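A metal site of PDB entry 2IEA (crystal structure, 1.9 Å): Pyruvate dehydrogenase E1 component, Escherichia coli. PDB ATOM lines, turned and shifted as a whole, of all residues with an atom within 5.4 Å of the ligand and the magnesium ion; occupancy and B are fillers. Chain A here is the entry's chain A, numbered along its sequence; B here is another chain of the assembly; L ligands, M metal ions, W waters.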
ATOM      1  N   HIS A 106      -0.465  35.723 -18.694  1.00  0.00           N
ATOM      2  CA  HIS A 106      -1.443  34.635 -18.569  1.00  0.00           C
ATOM      3  C   HIS A 106      -2.835  35.110 -18.159  1.00  0.00           C
ATOM      4  O   HIS A 106      -2.991  36.197 -17.582  1.00  0.00           O
ATOM      5  CB  HIS A 106      -0.943  33.629 -17.532  1.00  0.00           C
ATOM      6  CG  HIS A 106       0.505  33.280 -17.692  1.00  0.00           C
ATOM      7  ND1 HIS A 106       0.932  32.111 -18.289  1.00  0.00           N
ATOM      8  CD2 HIS A 106       1.630  33.951 -17.337  1.00  0.00           C
ATOM      9  CE1 HIS A 106       2.246  32.071 -18.302  1.00  0.00           C
ATOM     10  NE2 HIS A 106       2.700  33.176 -17.737  1.00  0.00           N
ATOM     11  N   SER A 109      -4.999  30.962 -15.402  1.00  0.00           N
ATOM     12  CA  SER A 109      -4.764  30.715 -13.979  1.00  0.00           C
ATOM     13  C   SER A 109      -5.540  31.658 -13.070  1.00  0.00           C
ATOM     14  O   SER A 109      -6.214  31.204 -12.153  1.00  0.00           O
ATOM     15  CB  SER A 109      -3.276  30.816 -13.667  1.00  0.00           C
ATOM     16  OG  SER A 109      -3.037  30.408 -12.328  1.00  0.00           O
ATOM     17  N   SER A 112      -9.111  30.886 -12.657  1.00  0.00           N
ATOM     18  CA  SER A 112      -9.432  29.762 -11.783  1.00  0.00           C
ATOM     19  C   SER A 112      -9.319  30.073 -10.295  1.00  0.00           C
ATOM     20  O   SER A 112      -9.970  29.437  -9.487  1.00  0.00           O
ATOM     21  CB  SER A 112      -8.549  28.541 -12.128  1.00  0.00           C
ATOM     22  OG  SER A 112      -7.214  28.701 -11.683  1.00  0.00           O
ATOM     23  N   GLN A 140       0.622  34.137  -6.072  1.00  0.00           N
ATOM     24  CA  GLN A 140       1.159  33.254  -7.107  1.00  0.00           C
ATOM     25  C   GLN A 140       1.581  34.187  -8.256  1.00  0.00           C
ATOM     26  O   GLN A 140       0.790  35.004  -8.728  1.00  0.00           O
ATOM     27  CB  GLN A 140       0.060  32.292  -7.568  1.00  0.00           C
ATOM     28  CG  GLN A 140       0.474  31.333  -8.671  1.00  0.00           C
ATOM     29  CD  GLN A 140      -0.667  30.421  -9.054  1.00  0.00           C
ATOM     30  OE1 GLN A 140      -1.829  30.846  -9.043  1.00  0.00           O
ATOM     31  NE2 GLN A 140      -0.363  29.173  -9.397  1.00  0.00           N
ATOM     32  N   HIS A 142       2.119  34.290 -11.694  1.00  0.00           N
ATOM     33  CA  HIS A 142       1.409  34.586 -12.935  1.00  0.00           C
ATOM     34  C   HIS A 142      -0.044  35.013 -12.848  1.00  0.00           C
ATOM     35  O   HIS A 142      -0.708  35.094 -13.877  1.00  0.00           O
ATOM     36  CB  HIS A 142       1.561  33.431 -13.926  1.00  0.00           C
ATOM     37  CG  HIS A 142       1.134  32.107 -13.388  1.00  0.00           C
ATOM     38  ND1 HIS A 142       1.812  31.466 -12.371  1.00  0.00           N
ATOM     39  CD2 HIS A 142       0.130  31.279 -13.751  1.00  0.00           C
ATOM     40  CE1 HIS A 142       1.232  30.302 -12.124  1.00  0.00           C
ATOM     41  NE2 HIS A 142       0.213  30.166 -12.949  1.00  0.00           N
ATOM     42  N   VAL A 192       7.470  33.927  -8.803  1.00  0.00           N
ATOM     43  CA  VAL A 192       7.424  33.231 -10.090  1.00  0.00           C
ATOM     44  C   VAL A 192       8.335  32.046 -10.259  1.00  0.00           C
ATOM     45  O   VAL A 192       8.014  31.151 -11.028  1.00  0.00           O
ATOM     46  CB  VAL A 192       7.708  34.108 -11.310  1.00  0.00           C
ATOM     47  CG1 VAL A 192       6.416  34.406 -11.991  1.00  0.00           C
ATOM     48  CG2 VAL A 192       8.489  35.340 -10.938  1.00  0.00           C
ATOM     49  N   SER A 193       9.485  32.043  -9.598  1.00  0.00           N
ATOM     50  CA  SER A 193      10.329  30.866  -9.706  1.00  0.00           C
ATOM     51  C   SER A 193       9.636  29.922  -8.743  1.00  0.00           C
ATOM     52  O   SER A 193       9.814  30.010  -7.528  1.00  0.00           O
ATOM     53  CB  SER A 193      11.748  31.149  -9.228  1.00  0.00           C
ATOM     54  OG  SER A 193      12.537  29.989  -9.396  1.00  0.00           O
ATOM     55  N   MET A 194       8.821  29.036  -9.290  1.00  0.00           N
ATOM     56  CA  MET A 194       8.065  28.117  -8.480  1.00  0.00           C
ATOM     57  C   MET A 194       8.870  27.280  -7.497  1.00  0.00           C
ATOM     58  O   MET A 194      10.008  26.899  -7.777  1.00  0.00           O
ATOM     59  CB  MET A 194       7.221  27.244  -9.390  1.00  0.00           C
ATOM     60  CG  MET A 194       6.148  28.079 -10.079  1.00  0.00           C
ATOM     61  SD  MET A 194       5.318  27.249 -11.408  1.00  0.00           S
ATOM     62  CE  MET A 194       4.375  28.629 -12.077  1.00  0.00           C
ATOM     63  N   GLY A 229       0.392  26.652  -6.788  1.00  0.00           N
ATOM     64  CA  GLY A 229      -0.301  25.902  -7.825  1.00  0.00           C
ATOM     65  C   GLY A 229      -0.092  24.444  -7.472  1.00  0.00           C
ATOM     66  O   GLY A 229       0.884  24.126  -6.783  1.00  0.00           O
ATOM     67  N   ASP A 230      -0.981  23.548  -7.915  1.00  0.00           N
ATOM     68  CA  ASP A 230      -0.780  22.139  -7.571  1.00  0.00           C
ATOM     69  C   ASP A 230       0.398  21.541  -8.329  1.00  0.00           C
ATOM     70  O   ASP A 230       1.136  20.713  -7.793  1.00  0.00           O
ATOM     71  CB  ASP A 230      -2.083  21.315  -7.765  1.00  0.00           C
ATOM     72  CG  ASP A 230      -2.753  21.550  -9.106  1.00  0.00           C
ATOM     73  OD1 ASP A 230      -3.888  21.062  -9.300  1.00  0.00           O
ATOM     74  OD2 ASP A 230      -2.158  22.203  -9.973  1.00  0.00           O
ATOM     75  N   GLY A 231       0.595  21.964  -9.578  1.00  0.00           N
ATOM     76  CA  GLY A 231       1.728  21.475 -10.344  1.00  0.00           C
ATOM     77  C   GLY A 231       3.036  21.897  -9.692  1.00  0.00           C
ATOM     78  O   GLY A 231       4.002  21.127  -9.658  1.00  0.00           O
ATOM     79  N   GLU A 232       3.055  23.118  -9.162  1.00  0.00           N
ATOM     80  CA  GLU A 232       4.227  23.667  -8.490  1.00  0.00           C
ATOM     81  C   GLU A 232       4.643  22.851  -7.275  1.00  0.00           C
ATOM     82  O   GLU A 232       5.820  22.845  -6.881  1.00  0.00           O
ATOM     83  CB  GLU A 232       3.947  25.127  -8.074  1.00  0.00           C
ATOM     84  CG  GLU A 232       4.791  25.635  -6.902  1.00  0.00           C
ATOM     85  CD  GLU A 232       4.602  27.124  -6.652  1.00  0.00           C
ATOM     86  OE1 GLU A 232       3.470  27.627  -6.802  1.00  0.00           O
ATOM     87  OE2 GLU A 232       5.596  27.792  -6.289  1.00  0.00           O
ATOM     88  N   GLU A 235       7.856  20.720  -7.211  1.00  0.00           N
ATOM     89  CA  GLU A 235       9.209  21.226  -6.953  1.00  0.00           C
ATOM     90  C   GLU A 235       9.590  20.703  -5.576  1.00  0.00           C
ATOM     91  O   GLU A 235       8.801  20.796  -4.635  1.00  0.00           O
ATOM     92  CB  GLU A 235       9.219  22.768  -6.937  1.00  0.00           C
ATOM     93  CG  GLU A 235       8.936  23.435  -8.279  1.00  0.00           C
ATOM     94  CD  GLU A 235      10.097  23.362  -9.269  1.00  0.00           C
ATOM     95  OE1 GLU A 235      10.084  24.114 -10.255  1.00  0.00           O
ATOM     96  OE2 GLU A 235      11.021  22.544  -9.055  1.00  0.00           O
ATOM     97  N   ASN A 258      -3.981  25.987  -5.215  1.00  0.00           N
ATOM     98  CA  ASN A 258      -5.027  26.046  -6.226  1.00  0.00           C
ATOM     99  C   ASN A 258      -5.023  24.712  -6.966  1.00  0.00           C
ATOM    100  O   ASN A 258      -4.194  24.481  -7.856  1.00  0.00           O
ATOM    101  CB  ASN A 258      -4.776  27.197  -7.197  1.00  0.00           C
ATOM    102  CG  ASN A 258      -5.853  27.315  -8.249  1.00  0.00           C
ATOM    103  OD1 ASN A 258      -6.838  26.575  -8.208  1.00  0.00           O
ATOM    104  ND2 ASN A 258      -5.680  28.233  -9.179  1.00  0.00           N
ATOM    105  N   CYS A 259      -5.942  23.840  -6.584  1.00  0.00           N
ATOM    106  CA  CYS A 259      -6.014  22.526  -7.207  1.00  0.00           C
ATOM    107  C   CYS A 259      -6.932  22.465  -8.418  1.00  0.00           C
ATOM    108  O   CYS A 259      -8.070  22.012  -8.327  1.00  0.00           O
ATOM    109  CB  CYS A 259      -6.443  21.491  -6.173  1.00  0.00           C
ATOM    110  SG  CYS A 259      -5.274  21.342  -4.791  1.00  0.00           S
ATOM    111  N   ASN A 260      -6.438  22.960  -9.564  1.00  0.00           N
ATOM    112  CA  ASN A 260      -7.225  22.903 -10.783  1.00  0.00           C
ATOM    113  C   ASN A 260      -6.867  21.610 -11.511  1.00  0.00           C
ATOM    114  O   ASN A 260      -7.311  21.365 -12.637  1.00  0.00           O
ATOM    115  CB  ASN A 260      -6.985  24.135 -11.664  1.00  0.00           C
ATOM    116  CG  ASN A 260      -5.529  24.488 -11.797  1.00  0.00           C
ATOM    117  OD1 ASN A 260      -4.681  23.612 -11.858  1.00  0.00           O
ATOM    118  ND2 ASN A 260      -5.228  25.777 -11.845  1.00  0.00           N
ATOM    119  N   LEU A 261      -6.057  20.797 -10.842  1.00  0.00           N
ATOM    120  CA  LEU A 261      -5.625  19.490 -11.350  1.00  0.00           C
ATOM    121  C   LEU A 261      -4.672  19.507 -12.539  1.00  0.00           C
ATOM    122  O   LEU A 261      -4.260  18.450 -13.018  1.00  0.00           O
ATOM    123  CB  LEU A 261      -6.850  18.645 -11.712  1.00  0.00           C
ATOM    124  CG  LEU A 261      -8.007  18.568 -10.719  1.00  0.00           C
ATOM    125  CD1 LEU A 261      -9.139  17.742 -11.309  1.00  0.00           C
ATOM    126  CD2 LEU A 261      -7.549  17.965  -9.407  1.00  0.00           C
ATOM    127  N   GLN A 262      -4.302  20.701 -13.005  1.00  0.00           N
ATOM    128  CA  GLN A 262      -3.433  20.786 -14.172  1.00  0.00           C
ATOM    129  C   GLN A 262      -2.208  21.667 -13.997  1.00  0.00           C
ATOM    130  O   GLN A 262      -2.221  22.631 -13.260  1.00  0.00           O
ATOM    131  CB  GLN A 262      -4.232  21.350 -15.358  1.00  0.00           C
ATOM    132  CG  GLN A 262      -5.641  20.814 -15.487  1.00  0.00           C
ATOM    133  CD  GLN A 262      -6.515  21.671 -16.396  1.00  0.00           C
ATOM    134  OE1 GLN A 262      -7.710  21.422 -16.531  1.00  0.00           O
ATOM    135  NE2 GLN A 262      -5.904  22.669 -17.029  1.00  0.00           N
ATOM    136  N   ARG A 263      -1.127  21.307 -14.695  1.00  0.00           N
ATOM    137  CA  ARG A 263       0.064  22.145 -14.654  1.00  0.00           C
ATOM    138  C   ARG A 263      -0.008  22.869 -15.993  1.00  0.00           C
ATOM    139  O   ARG A 263      -1.099  23.126 -16.484  1.00  0.00           O
ATOM    140  CB  ARG A 263       1.344  21.306 -14.512  1.00  0.00           C
ATOM    141  CG  ARG A 263       1.364  19.973 -15.214  1.00  0.00           C
ATOM    142  CD  ARG A 263       2.678  19.259 -14.904  1.00  0.00           C
ATOM    143  NE  ARG A 263       2.704  17.908 -15.461  1.00  0.00           N
ATOM    144  CZ  ARG A 263       2.681  17.634 -16.757  1.00  0.00           C
ATOM    145  NH1 ARG A 263       2.696  16.376 -17.174  1.00  0.00           N
ATOM    146  NH2 ARG A 263       2.651  18.617 -17.641  1.00  0.00           N
ATOM    147  N   LEU A 264       1.124  23.192 -16.606  1.00  0.00           N
ATOM    148  CA  LEU A 264       1.064  23.908 -17.878  1.00  0.00           C
ATOM    149  C   LEU A 264       0.664  23.033 -19.060  1.00  0.00           C
ATOM    150  O   LEU A 264      -0.378  23.280 -19.686  1.00  0.00           O
ATOM    151  CB  LEU A 264       2.409  24.604 -18.154  1.00  0.00           C
ATOM    152  CG  LEU A 264       2.430  25.798 -19.134  1.00  0.00           C
ATOM    153  CD1 LEU A 264       2.386  25.320 -20.566  1.00  0.00           C
ATOM    154  CD2 LEU A 264       1.276  26.728 -18.827  1.00  0.00           C
ATOM    155  N   VAL A 268      -1.485  17.307 -13.430  1.00  0.00           N
ATOM    156  CA  VAL A 268      -0.373  16.987 -12.556  1.00  0.00           C
ATOM    157  C   VAL A 268      -0.203  15.472 -12.494  1.00  0.00           C
ATOM    158  O   VAL A 268       0.900  14.953 -12.656  1.00  0.00           O
ATOM    159  CB  VAL A 268      -0.609  17.536 -11.133  1.00  0.00           C
ATOM    160  CG1 VAL A 268       0.662  17.400 -10.307  1.00  0.00           C
ATOM    161  CG2 VAL A 268      -1.047  18.992 -11.207  1.00  0.00           C
ATOM    162  N   LYS A 392      -9.464  25.281 -14.312  1.00  0.00           N
ATOM    163  CA  LYS A 392      -8.464  26.120 -14.974  1.00  0.00           C
ATOM    164  C   LYS A 392      -9.072  26.719 -16.238  1.00  0.00           C
ATOM    165  O   LYS A 392      -9.706  26.025 -17.024  1.00  0.00           O
ATOM    166  CB  LYS A 392      -7.222  25.282 -15.311  1.00  0.00           C
ATOM    167  CG  LYS A 392      -6.026  26.101 -15.756  1.00  0.00           C
ATOM    168  CD  LYS A 392      -4.743  25.281 -15.678  1.00  0.00           C
ATOM    169  CE  LYS A 392      -3.564  26.047 -16.232  1.00  0.00           C
ATOM    170  NZ  LYS A 392      -3.786  26.364 -17.668  1.00  0.00           N
ATOM    171  N   ASP A 609      19.128  30.029  -6.780  1.00  0.00           N
ATOM    172  CA  ASP A 609      17.886  30.623  -7.249  1.00  0.00           C
ATOM    173  C   ASP A 609      17.283  31.505  -6.153  1.00  0.00           C
ATOM    174  O   ASP A 609      16.641  32.511  -6.433  1.00  0.00           O
ATOM    175  CB  ASP A 609      16.893  29.544  -7.670  1.00  0.00           C
ATOM    176  CG  ASP A 609      15.958  30.005  -8.791  1.00  0.00           C
ATOM    177  OD1 ASP A 609      14.884  29.399  -8.938  1.00  0.00           O
ATOM    178  OD2 ASP A 609      16.316  30.943  -9.534  1.00  0.00           O
ATOM    179  N   ALA B 520      10.488  19.518 -18.205  1.00  0.00           N
ATOM    180  CA  ALA B 520       9.902  19.794 -16.912  1.00  0.00           C
ATOM    181  C   ALA B 520       8.590  20.539 -17.151  1.00  0.00           C
ATOM    182  O   ALA B 520       8.545  21.760 -17.082  1.00  0.00           O
ATOM    183  CB  ALA B 520      10.859  20.639 -16.071  1.00  0.00           C
ATOM    184  N   ASP B 521       7.551  19.772 -17.441  1.00  0.00           N
ATOM    185  CA  ASP B 521       6.213  20.286 -17.738  1.00  0.00           C
ATOM    186  C   ASP B 521       6.159  20.919 -19.123  1.00  0.00           C
ATOM    187  O   ASP B 521       5.633  20.325 -20.064  1.00  0.00           O
ATOM    188  CB  ASP B 521       5.762  21.312 -16.685  1.00  0.00           C
ATOM    189  CG  ASP B 521       4.353  21.824 -16.943  1.00  0.00           C
ATOM    190  OD1 ASP B 521       3.637  21.217 -17.771  1.00  0.00           O
ATOM    191  OD2 ASP B 521       3.957  22.834 -16.325  1.00  0.00           O
ATOM    192  N   GLU B 522       6.716  22.125 -19.230  1.00  0.00           N
ATOM    193  CA  GLU B 522       6.739  22.873 -20.489  1.00  0.00           C
ATOM    194  C   GLU B 522       7.384  22.141 -21.659  1.00  0.00           C
ATOM    195  O   GLU B 522       8.573  21.817 -21.631  1.00  0.00           O
ATOM    196  CB  GLU B 522       7.459  24.209 -20.301  1.00  0.00           C
ATOM    197  CG  GLU B 522       6.570  25.443 -20.286  1.00  0.00           C
ATOM    198  CD  GLU B 522       5.987  25.740 -18.922  1.00  0.00           C
ATOM    199  OE1 GLU B 522       5.461  24.795 -18.290  1.00  0.00           O
ATOM    200  OE2 GLU B 522       6.057  26.902 -18.475  1.00  0.00           O
ATOM    201  N   ILE B 569       6.798  20.159 -13.062  1.00  0.00           N
ATOM    202  CA  ILE B 569       7.450  21.350 -12.545  1.00  0.00           C
ATOM    203  C   ILE B 569       8.403  20.909 -11.451  1.00  0.00           C
ATOM    204  O   ILE B 569       8.137  21.063 -10.249  1.00  0.00           O
ATOM    205  CB  ILE B 569       6.405  22.338 -11.986  1.00  0.00           C
ATOM    206  CG1 ILE B 569       5.280  22.525 -13.019  1.00  0.00           C
ATOM    207  CG2 ILE B 569       7.064  23.675 -11.679  1.00  0.00           C
ATOM    208  CD1 ILE B 569       4.169  23.470 -12.584  1.00  0.00           C
ATOM    209  N   GLU B 571      12.569  20.892 -11.709  1.00  0.00           N
ATOM    210  CA  GLU B 571      13.851  20.918 -12.394  1.00  0.00           C
ATOM    211  C   GLU B 571      14.896  19.991 -11.780  1.00  0.00           C
ATOM    212  O   GLU B 571      15.674  19.371 -12.493  1.00  0.00           O
ATOM    213  CB  GLU B 571      14.408  22.345 -12.462  1.00  0.00           C
ATOM    214  CG  GLU B 571      13.739  23.246 -13.496  1.00  0.00           C
ATOM    215  CD  GLU B 571      12.403  23.794 -13.042  1.00  0.00           C
ATOM    216  OE1 GLU B 571      12.081  23.676 -11.838  1.00  0.00           O
ATOM    217  OE2 GLU B 571      11.679  24.356 -13.887  1.00  0.00           O
ATOM    218  N   TYR B 599      13.848  26.071 -18.972  1.00  0.00           N
ATOM    219  CA  TYR B 599      14.163  27.501 -18.999  1.00  0.00           C
ATOM    220  C   TYR B 599      15.586  27.624 -18.468  1.00  0.00           C
ATOM    221  O   TYR B 599      15.841  27.253 -17.328  1.00  0.00           O
ATOM    222  CB  TYR B 599      13.215  28.289 -18.107  1.00  0.00           C
ATOM    223  CG  TYR B 599      11.822  28.496 -18.674  1.00  0.00           C
ATOM    224  CD1 TYR B 599      10.885  27.467 -18.644  1.00  0.00           C
ATOM    225  CD2 TYR B 599      11.431  29.725 -19.182  1.00  0.00           C
ATOM    226  CE1 TYR B 599       9.576  27.668 -19.111  1.00  0.00           C
ATOM    227  CE2 TYR B 599      10.150  29.947 -19.645  1.00  0.00           C
ATOM    228  CZ  TYR B 599       9.219  28.909 -19.606  1.00  0.00           C
ATOM    229  OH  TYR B 599       7.941  29.132 -20.048  1.00  0.00           O
ATOM    230  N   PHE B 602      16.566  28.351 -14.844  1.00  0.00           N
ATOM    231  CA  PHE B 602      16.339  27.332 -13.821  1.00  0.00           C
ATOM    232  C   PHE B 602      17.268  26.137 -13.965  1.00  0.00           C
ATOM    233  O   PHE B 602      16.942  25.035 -13.522  1.00  0.00           O
ATOM    234  CB  PHE B 602      14.885  26.877 -13.858  1.00  0.00           C
ATOM    235  CG  PHE B 602      13.903  28.020 -13.735  1.00  0.00           C
ATOM    236  CD1 PHE B 602      12.794  28.080 -14.577  1.00  0.00           C
ATOM    237  CD2 PHE B 602      14.105  29.033 -12.822  1.00  0.00           C
ATOM    238  CE1 PHE B 602      11.910  29.155 -14.509  1.00  0.00           C
ATOM    239  CE2 PHE B 602      13.232  30.109 -12.738  1.00  0.00           C
ATOM    240  CZ  PHE B 602      12.131  30.180 -13.586  1.00  0.00           C
ATOM    241  N   ARG B 606      19.463  27.052 -10.316  1.00  0.00           N
ATOM    242  CA  ARG B 606      18.511  26.318  -9.483  1.00  0.00           C
ATOM    243  C   ARG B 606      18.943  24.918  -9.059  1.00  0.00           C
ATOM    244  O   ARG B 606      18.604  24.478  -7.954  1.00  0.00           O
ATOM    245  CB  ARG B 606      17.169  26.253 -10.224  1.00  0.00           C
ATOM    246  CG  ARG B 606      16.041  25.512  -9.497  1.00  0.00           C
ATOM    247  CD  ARG B 606      15.721  26.117  -8.138  1.00  0.00           C
ATOM    248  NE  ARG B 606      14.514  25.520  -7.584  1.00  0.00           N
ATOM    249  CZ  ARG B 606      13.288  26.030  -7.727  1.00  0.00           C
ATOM    250  NH1 ARG B 606      13.104  27.163  -8.394  1.00  0.00           N
ATOM    251  NH2 ARG B 606      12.239  25.376  -7.247  1.00  0.00           N
ATOM    252  N   HIS B 640      13.408  35.317 -14.922  1.00  0.00           N
ATOM    253  CA  HIS B 640      13.448  34.427 -16.077  1.00  0.00           C
ATOM    254  C   HIS B 640      14.546  34.792 -17.076  1.00  0.00           C
ATOM    255  O   HIS B 640      15.103  33.907 -17.742  1.00  0.00           O
ATOM    256  CB  HIS B 640      12.121  34.482 -16.846  1.00  0.00           C
ATOM    257  CG  HIS B 640      10.975  33.809 -16.159  1.00  0.00           C
ATOM    258  ND1 HIS B 640      10.340  34.350 -15.064  1.00  0.00           N
ATOM    259  CD2 HIS B 640      10.334  32.654 -16.438  1.00  0.00           C
ATOM    260  CE1 HIS B 640       9.343  33.556 -14.702  1.00  0.00           C
ATOM    261  NE2 HIS B 640       9.327  32.520 -15.514  1.00  0.00           N
HETATM  262  N1  LIG L   1       9.842  26.400 -13.438  1.00  0.00           N
HETATM  263  C1  LIG L   1       9.925  27.351 -12.436  1.00  0.00           C
HETATM  264  C2  LIG L   1      10.923  27.122 -11.359  1.00  0.00           C
HETATM  265  N2  LIG L   1       9.154  28.449 -12.415  1.00  0.00           N
HETATM  266  C3  LIG L   1       8.236  28.652 -13.451  1.00  0.00           C
HETATM  267  N3  LIG L   1       7.520  29.762 -13.371  1.00  0.00           N
HETATM  268  C4  LIG L   1       8.126  27.668 -14.543  1.00  0.00           C
HETATM  269  C5  LIG L   1       8.948  26.563 -14.477  1.00  0.00           C
HETATM  270  C6  LIG L   1       7.240  27.848 -15.774  1.00  0.00           C
HETATM  271  N4  LIG L   1       5.745  27.787 -15.501  1.00  0.00           N
HETATM  272  C7  LIG L   1       4.949  28.842 -15.584  1.00  0.00           C
HETATM  273  S1  LIG L   1       3.334  28.467 -15.347  1.00  0.00           S
HETATM  274  C8  LIG L   1       3.713  26.801 -15.121  1.00  0.00           C
HETATM  275  C9  LIG L   1       5.056  26.580 -15.235  1.00  0.00           C
HETATM  276  C10 LIG L   1       5.783  25.264 -15.117  1.00  0.00           C
HETATM  277  C11 LIG L   1       2.654  25.804 -14.781  1.00  0.00           C
HETATM  278  C12 LIG L   1       1.818  26.280 -13.624  1.00  0.00           C
HETATM  279  O1  LIG L   1       1.203  25.122 -13.018  1.00  0.00           O
HETATM  280  P1  LIG L   1       0.622  25.162 -11.521  1.00  0.00           P
HETATM  281  O2  LIG L   1       1.740  25.393 -10.574  1.00  0.00           O
HETATM  282  O3  LIG L   1      -0.204  23.949 -11.342  1.00  0.00           O
HETATM  283  O4  LIG L   1      -0.333  26.463 -11.511  1.00  0.00           O
HETATM  284  P2  LIG L   1      -1.649  26.949 -12.305  1.00  0.00           P
HETATM  285  O5  LIG L   1      -1.218  27.964 -13.303  1.00  0.00           O
HETATM  286  O6  LIG L   1      -2.563  27.641 -11.249  1.00  0.00           O
HETATM  287  O7  LIG L   1      -2.333  25.757 -12.848  1.00  0.00           O
HETATM  288 MG    MG M   1      -2.652  23.783 -11.361  1.00  0.00          MG
HETATM  289  O   HOH W   1       4.821  29.379 -18.840  1.00  0.00           O
HETATM  290  O   HOH W   2       2.104  27.878  -9.369  1.00  0.00           O
HETATM  291  O   HOH W   3      -2.777  25.350  -9.763  1.00  0.00           O
HETATM  292  O   HOH W   4       9.001  23.507 -14.800  1.00  0.00           O
HETATM  293  O   HOH W   5       6.673  31.451 -15.855  1.00  0.00           O
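A ring nitrogen (NE2) of His 142 sits at hydrogen-bond distance from an oxygen (O5) of the ligand.
N3 of the ligand lies within hydrogen-bond range of O of Val 192 (2.8 Å).
An oxygen (O3) of the ligand sits close to the backbone NH (N) of Gly 231 (2.8 Å).
The side-chain carboxylate of Glu 571 of chain B lies within hydrogen-bond range of a nitrogen (N1) of the ligand.
O2 of the ligand lies within hydrogen-bond range of N of Glu 232 (3.0 Å).
An oxygen (O6) of the ligand sits at hydrogen-bond distance from the side-chain hydroxyl (OG) of Ser 109, at 3.0 Å.
N of Met 194 is in hydrogen-bond range of N2 of the ligand, at 3.2 Å.
NE2 of Gln 140 lies within hydrogen-bond range of O6 of the ligand (3.3 Å).
The side-chain carboxylate (OD1) of Asp 230 lies within hydrogen-bond range of the backbone NH (N) of Leu 261 (2.7 Å).
OE1 of Glu 232 lies within hydrogen-bond range of N of Gly 229, 3.2 Å away.
The backbone carbonyl oxygen (O) of Ser 109 sits at hydrogen-bond distance from the side-chain hydroxyl (OG) of Ser 112 (2.7 Å).
The side-chain hydroxyl of Tyr 599 of chain B lies within hydrogen-bond range of the side-chain carboxylate of Glu 522 of chain B.
The side-chain carboxylate of Asp 521 of chain B sits at hydrogen-bond distance from the backbone NH of Leu 264, 2.9 Å away.
O of Ile 569 of chain B lies within hydrogen-bond range of N of Glu 235, 3.1 Å away.
OG of Ser 193 sits at hydrogen-bond distance from NH1 of Arg 606 of chain B (3.1 Å).
The side-chain amide nitrogen (ND2) of Asn 258 is in hydrogen-bond range of the side-chain hydroxyl (OG) of Ser 112 (3.0 Å).
The side-chain carboxylate of Glu 522 of chain B sits close to a nitrogen (N4) of the ligand.
Residues that only touch the ligand: Ser 193 (3.8 Å), Gly 229 (3.5 Å), Glu 235 (3.3 Å), Asn 258 (3.8 Å), Arg 263 (3.6 Å), Leu 264 (3.5 Å), Lys 392 (3.6 Å), Asp 521 of chain B (3.3 Å), Ile 569 of chain B (3.4 Å), Phe 602 of chain B (3.4 Å), Arg 606 of chain B (3.7 Å) and His 640 of chain B (3.9 Å).
Of the 32 residues printed, 24 come within 4 Å of the ligand.
Asn 258 touches the magnesium ion (O to MG, 3.9 Å).
Of the 32 residues printed, 4 come within 4 Å of the magnesium ion.
The nearest printed residue that does not touch the magnesium ion is Gly 231 (4.1 Å).
The side-chain amide oxygen (OD1) of Asn 260 is bound to the magnesium ion (2.1 Å).
The magnesium ion is bound by OD2 of Asp 230 (2.2 Å).
Water W3 is bound to the magnesium ion, 2.2 Å away.
The magnesium ion is bound by the backbone carbonyl oxygen (O) of Gln 262, 2.3 Å away.
O3 of the ligand binds the magnesium ion.
The magnesium ion is bound by O7 of the ligand (2.5 Å).
Water W3 lies within hydrogen-bond range of O of Asn 258 (2.5 Å), O6 of the ligand (2.7 Å), N of Asp 230 (3.1 Å) and ND2 of Asn 260 (3.2 Å).
Water W2 lies within hydrogen-bond range of an oxygen (O2) of the ligand (2.8 Å), the side-chain amide nitrogen (NE2) of Gln 140 (2.8 Å), the side-chain carboxylate (OE1) of Glu 232 (2.9 Å) and the backbone NH (N) of Gly 229 (3.3 Å).
Water W5 bridges a ring nitrogen (NE2) of His 640 of chain B (2.9 Å) and a nitrogen (N3) of the ligand (3.1 Å).
Water W1 lies within hydrogen-bond range of the side-chain carboxylate (OE2) of Glu 522 of chain B (2.8 Å) and the side-chain hydroxyl (OH) of Tyr 599 of chain B (3.4 Å).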
